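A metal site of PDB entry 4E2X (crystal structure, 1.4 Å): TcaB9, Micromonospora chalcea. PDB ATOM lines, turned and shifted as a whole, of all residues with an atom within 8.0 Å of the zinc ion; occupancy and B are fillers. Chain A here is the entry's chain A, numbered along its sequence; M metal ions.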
ATOM      1  N   ALA A  14      12.523  17.786  18.513  1.00  0.00           N
ATOM      2  CA  ALA A  14      13.730  17.779  17.687  1.00  0.00           C
ATOM      3  C   ALA A  14      13.932  16.382  17.077  1.00  0.00           C
ATOM      4  O   ALA A  14      13.853  15.371  17.782  1.00  0.00           O
ATOM      5  CB  ALA A  14      14.966  18.150  18.529  1.00  0.00           C
ATOM      6  N   CYS A  15      14.199  16.331  15.774  1.00  0.00           N
ATOM      7  CA  CYS A  15      14.521  15.062  15.114  1.00  0.00           C
ATOM      8  C   CYS A  15      15.654  14.333  15.861  1.00  0.00           C
ATOM      9  O   CYS A  15      16.708  14.912  16.123  1.00  0.00           O
ATOM     10  CB  CYS A  15      14.877  15.301  13.645  1.00  0.00           C
ATOM     11  SG  CYS A  15      15.462  13.813  12.804  1.00  0.00           S
ATOM     12  N   ARG A  16      15.442  13.050  16.188  1.00  0.00           N
ATOM     13  CA  ARG A  16      16.429  12.172  16.795  1.00  0.00           C
ATOM     14  C   ARG A  16      17.641  11.816  15.930  1.00  0.00           C
ATOM     15  O   ARG A  16      18.669  11.335  16.432  1.00  0.00           O
ATOM     16  CB  ARG A  16      15.795  10.970  17.520  1.00  0.00           C
ATOM     17  CG  ARG A  16      15.164  11.311  18.844  1.00  0.00           C
ATOM     18  CD  ARG A  16      16.335  11.450  19.859  1.00  0.00           C
ATOM     19  NE  ARG A  16      16.093  10.632  21.058  1.00  0.00           N
ATOM     20  CZ  ARG A  16      17.024  10.098  21.839  1.00  0.00           C
ATOM     21  NH1 ARG A  16      16.633   9.404  22.893  1.00  0.00           N
ATOM     22  NH2 ARG A  16      18.328  10.248  21.590  1.00  0.00           N
ATOM     23  N   VAL A  17      17.497  12.089  14.632  1.00  0.00           N
ATOM     24  CA  VAL A  17      18.599  11.835  13.736  1.00  0.00           C
ATOM     25  C   VAL A  17      19.450  13.102  13.565  1.00  0.00           C
ATOM     26  O   VAL A  17      20.691  13.027  13.710  1.00  0.00           O
ATOM     27  CB  VAL A  17      18.139  11.302  12.349  1.00  0.00           C
ATOM     28  CG1 VAL A  17      19.297  11.186  11.400  1.00  0.00           C
ATOM     29  CG2 VAL A  17      17.505   9.924  12.540  1.00  0.00           C
ATOM     30  N   CYS A  18      18.845  14.244  13.278  1.00  0.00           N
ATOM     31  CA  CYS A  18      19.667  15.368  12.828  1.00  0.00           C
ATOM     32  C   CYS A  18      19.442  16.618  13.685  1.00  0.00           C
ATOM     33  O   CYS A  18      20.131  17.616  13.482  1.00  0.00           O
ATOM     34  CB  CYS A  18      19.488  15.717  11.333  1.00  0.00           C
ATOM     35  SG  CYS A  18      17.853  16.459  10.987  1.00  0.00           S
ATOM     36  N   GLY A  19      18.462  16.607  14.586  1.00  0.00           N
ATOM     37  CA  GLY A  19      18.072  17.797  15.351  1.00  0.00           C
ATOM     38  C   GLY A  19      17.130  18.763  14.651  1.00  0.00           C
ATOM     39  O   GLY A  19      16.719  19.773  15.236  1.00  0.00           O
ATOM     40  N   GLY A  20      16.754  18.448  13.413  1.00  0.00           N
ATOM     41  CA  GLY A  20      15.798  19.230  12.634  1.00  0.00           C
ATOM     42  C   GLY A  20      14.449  19.295  13.328  1.00  0.00           C
ATOM     43  O   GLY A  20      14.204  18.605  14.322  1.00  0.00           O
ATOM     44  N   GLY A  21      13.542  20.108  12.797  1.00  0.00           N
ATOM     45  CA  GLY A  21      12.211  20.147  13.381  1.00  0.00           C
ATOM     46  C   GLY A  21      11.247  19.111  12.858  1.00  0.00           C
ATOM     47  O   GLY A  21      11.180  18.872  11.637  1.00  0.00           O
ATOM     48  N   VAL A  22      10.530  18.465  13.781  1.00  0.00           N
ATOM     49  CA  VAL A  22       9.553  17.460  13.363  1.00  0.00           C
ATOM     50  C   VAL A  22       8.141  18.028  13.318  1.00  0.00           C
ATOM     51  O   VAL A  22       7.645  18.500  14.347  1.00  0.00           O
ATOM     52  CB  VAL A  22       9.612  16.242  14.320  1.00  0.00           C
ATOM     53  CG1 VAL A  22       8.557  15.197  14.026  1.00  0.00           C
ATOM     54  CG2 VAL A  22      10.995  15.566  14.231  1.00  0.00           C
ATOM     55  N   ARG A  55       7.270  14.265  10.597  1.00  0.00           N
ATOM     56  CA  ARG A  55       8.405  14.120   9.726  1.00  0.00           C
ATOM     57  C   ARG A  55       9.403  15.227   9.991  1.00  0.00           C
ATOM     58  O   ARG A  55       8.992  16.401  10.079  1.00  0.00           O
ATOM     59  CB  ARG A  55       7.928  14.097   8.266  1.00  0.00           C
ATOM     60  CG  ARG A  55       9.071  13.859   7.307  1.00  0.00           C
ATOM     61  CD  ARG A  55       8.891  14.450   5.920  1.00  0.00           C
ATOM     62  NE  ARG A  55       9.045  15.902   5.962  1.00  0.00           N
ATOM     63  CZ  ARG A  55       8.871  16.731   4.939  1.00  0.00           C
ATOM     64  NH1 ARG A  55       9.038  18.043   5.112  1.00  0.00           N
ATOM     65  NH2 ARG A  55       8.502  16.266   3.755  1.00  0.00           N
ATOM     66  N   CYS A  56      10.693  14.898  10.086  1.00  0.00           N
ATOM     67  CA  CYS A  56      11.714  15.927  10.202  1.00  0.00           C
ATOM     68  C   CYS A  56      11.772  16.798   8.944  1.00  0.00           C
ATOM     69  O   CYS A  56      11.714  16.281   7.829  1.00  0.00           O
ATOM     70  CB  CYS A  56      13.059  15.241  10.419  1.00  0.00           C
ATOM     71  SG  CYS A  56      14.357  16.510  10.417  1.00  0.00           S
ATOM     72  N   ASP A  57      11.888  18.114   9.145  1.00  0.00           N
ATOM     73  CA  ASP A  57      12.004  19.116   8.080  1.00  0.00           C
ATOM     74  C   ASP A  57      13.319  19.016   7.308  1.00  0.00           C
ATOM     75  O   ASP A  57      13.435  19.530   6.194  1.00  0.00           O
ATOM     76  CB  ASP A  57      12.098  20.526   8.695  1.00  0.00           C
ATOM     77  CG  ASP A  57      10.758  21.079   9.046  1.00  0.00           C
ATOM     78  OD1 ASP A  57       9.791  20.486   8.549  1.00  0.00           O
ATOM     79  OD2 ASP A  57      10.717  22.072   9.811  1.00  0.00           O
ATOM     80  N   SER A  58      14.335  18.395   7.885  1.00  0.00           N
ATOM     81  CA  SER A  58      15.658  18.501   7.318  1.00  0.00           C
ATOM     82  C   SER A  58      16.121  17.190   6.705  1.00  0.00           C
ATOM     83  O   SER A  58      16.775  17.217   5.668  1.00  0.00           O
ATOM     84  CB  SER A  58      16.641  18.898   8.404  1.00  0.00           C
ATOM     85  OG  SER A  58      16.228  20.167   8.858  1.00  0.00           O
ATOM     86  N   CYS A  59      15.846  16.054   7.338  1.00  0.00           N
ATOM     87  CA  CYS A  59      16.335  14.783   6.853  1.00  0.00           C
ATOM     88  C   CYS A  59      15.211  13.853   6.349  1.00  0.00           C
ATOM     89  O   CYS A  59      15.532  12.760   5.894  1.00  0.00           O
ATOM     90  CB  CYS A  59      17.194  14.096   7.923  1.00  0.00           C
ATOM     91  SG  CYS A  59      16.203  13.330   9.207  1.00  0.00           S
ATOM     92  N   GLU A  60      13.953  14.285   6.482  1.00  0.00           N
ATOM     93  CA  GLU A  60      12.791  13.511   6.057  1.00  0.00           C
ATOM     94  C   GLU A  60      12.472  12.246   6.864  1.00  0.00           C
ATOM     95  O   GLU A  60      11.609  11.474   6.456  1.00  0.00           O
ATOM     96  CB  GLU A  60      12.679  13.246   4.539  1.00  0.00           C
ATOM     97  CG  GLU A  60      12.690  14.602   3.780  1.00  0.00           C
ATOM     98  CD  GLU A  60      12.611  14.365   2.295  1.00  0.00           C
ATOM     99  OE1 GLU A  60      11.487  14.093   1.848  1.00  0.00           O
ATOM    100  OE2 GLU A  60      13.666  14.435   1.608  1.00  0.00           O
ATOM    101  N   MET A  61      13.075  12.086   8.038  1.00  0.00           N
ATOM    102  CA  MET A  61      12.859  10.920   8.881  1.00  0.00           C
ATOM    103  C   MET A  61      11.476  11.084   9.535  1.00  0.00           C
ATOM    104  O   MET A  61      11.215  12.065  10.229  1.00  0.00           O
ATOM    105  CB  MET A  61      13.910  10.795   9.967  1.00  0.00           C
ATOM    106  CG  MET A  61      13.710   9.567  10.838  1.00  0.00           C
ATOM    107  SD  MET A  61      13.832   7.992   9.906  1.00  0.00           S
ATOM    108  CE  MET A  61      15.628   7.865   9.770  1.00  0.00           C
ATOM    109  N   VAL A  62      10.647  10.067   9.295  1.00  0.00           N
ATOM    110  CA  VAL A  62       9.337   9.954   9.914  1.00  0.00           C
ATOM    111  C   VAL A  62       9.531   9.248  11.261  1.00  0.00           C
ATOM    112  O   VAL A  62      10.139   8.192  11.339  1.00  0.00           O
ATOM    113  CB  VAL A  62       8.356   9.192   8.984  1.00  0.00           C
ATOM    114  CG1 VAL A  62       7.053   8.905   9.675  1.00  0.00           C
ATOM    115  CG2 VAL A  62       8.105   9.979   7.662  1.00  0.00           C
ATOM    116  N   GLN A  63       8.970   9.831  12.313  1.00  0.00           N
ATOM    117  CA  GLN A  63       9.243   9.429  13.684  1.00  0.00           C
ATOM    118  C   GLN A  63       8.104   9.832  14.614  1.00  0.00           C
ATOM    119  O   GLN A  63       7.426  10.827  14.367  1.00  0.00           O
ATOM    120  CB  GLN A  63      10.563   9.957  14.277  1.00  0.00           C
ATOM    121  CG  GLN A  63      10.639  11.489  14.356  1.00  0.00           C
ATOM    122  CD  GLN A  63      12.076  11.960  14.296  1.00  0.00           C
ATOM    123  OE1 GLN A  63      12.749  12.055  15.324  1.00  0.00           O
ATOM    124  NE2 GLN A  63      12.547  12.310  13.101  1.00  0.00           N
ATOM    125  N   PHE A 229      10.590   4.891  14.544  1.00  0.00           N
ATOM    126  CA  PHE A 229      10.885   5.327  13.194  1.00  0.00           C
ATOM    127  C   PHE A 229      10.105   4.546  12.165  1.00  0.00           C
ATOM    128  O   PHE A 229       9.989   3.331  12.281  1.00  0.00           O
ATOM    129  CB  PHE A 229      12.401   5.200  12.854  1.00  0.00           C
ATOM    130  CG  PHE A 229      13.308   6.067  13.673  1.00  0.00           C
ATOM    131  CD1 PHE A 229      13.262   7.447  13.528  1.00  0.00           C
ATOM    132  CD2 PHE A 229      14.177   5.522  14.609  1.00  0.00           C
ATOM    133  CE1 PHE A 229      14.089   8.261  14.323  1.00  0.00           C
ATOM    134  CE2 PHE A 229      15.004   6.314  15.386  1.00  0.00           C
ATOM    135  CZ  PHE A 229      14.985   7.710  15.234  1.00  0.00           C
ATOM    136  N   SER A 235      15.125   8.656   3.941  1.00  0.00           N
ATOM    137  CA  SER A 235      15.619   9.006   5.280  1.00  0.00           C
ATOM    138  C   SER A 235      16.796   8.172   5.768  1.00  0.00           C
ATOM    139  O   SER A 235      17.691   8.680   6.420  1.00  0.00           O
ATOM    140  CB  SER A 235      14.448   8.929   6.258  1.00  0.00           C
ATOM    141  OG  SER A 235      13.928   7.638   6.434  1.00  0.00           O
ATOM    142  N   MET A 239      20.380   9.442   7.024  1.00  0.00           N
ATOM    143  CA  MET A 239      20.881   9.022   8.316  1.00  0.00           C
ATOM    144  C   MET A 239      22.259   8.398   8.265  1.00  0.00           C
ATOM    145  O   MET A 239      23.130   8.708   9.082  1.00  0.00           O
ATOM    146  CB  MET A 239      19.888   8.022   8.917  1.00  0.00           C
ATOM    147  CG  MET A 239      20.325   7.503  10.304  1.00  0.00           C
ATOM    148  SD  MET A 239      19.131   6.348  11.031  1.00  0.00           S
ATOM    149  CE  MET A 239      19.146   4.996   9.849  1.00  0.00           C
ATOM    150  N   ARG A 242      24.893  11.142   7.356  1.00  0.00           N
ATOM    151  CA  ARG A 242      25.158  12.095   8.438  1.00  0.00           C
ATOM    152  C   ARG A 242      26.048  11.460   9.501  1.00  0.00           C
ATOM    153  O   ARG A 242      26.546  12.168  10.378  1.00  0.00           O
ATOM    154  CB  ARG A 242      23.855  12.601   9.072  1.00  0.00           C
ATOM    155  CG  ARG A 242      23.147  13.703   8.278  1.00  0.00           C
ATOM    156  CD  ARG A 242      21.653  13.784   8.628  1.00  0.00           C
ATOM    157  NE  ARG A 242      21.081  15.028   8.145  1.00  0.00           N
ATOM    158  CZ  ARG A 242      20.432  15.184   6.999  1.00  0.00           C
ATOM    159  NH1 ARG A 242      20.244  14.164   6.159  1.00  0.00           N
ATOM    160  NH2 ARG A 242      19.966  16.391   6.711  1.00  0.00           N
HETATM  161 ZN    ZN M   1      16.132  14.933  10.868  1.00  0.00          ZN
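N of Gly 20 sits close to SG of Cys 18 (3.3 Å). The side-chain sulfur (SG) of Cys 59 sits close to the backbone NH (N) of Met 61 (3.6 Å). The backbone NH (N) of Cys 15 is in hydrogen-bond range of the backbone carbonyl oxygen (O) of Gly 20. The backbone NH (N) of Val 17 lies close to the side-chain sulfur (SG) of Cys 15 (3.2 Å). The side-chain sulfur (SG) of Cys 15 sits close to the side-chain amide nitrogen (NE2) of Gln 63. The side-chain sulfur of Cys 56 sits close to the backbone NH of Ser 58. O of Met 61 lies within hydrogen-bond range of N of Cys 56 (2.9 Å).
Along chain A the residues within 4 Å of the zinc ion span positions 15 to 59. The nearest printed residue that does not touch the zinc ion is Gly 20 (4.4 Å).
The zinc ion is bound by the side-chain sulfur (SG) of Cys 18 (2.3 Å), the side-chain sulfur (SG) of Cys 59 (2.3 Å), the side-chain sulfur (SG) of Cys 15 (2.3 Å) and the side-chain sulfur (SG) of Cys 56 (2.4 Å).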
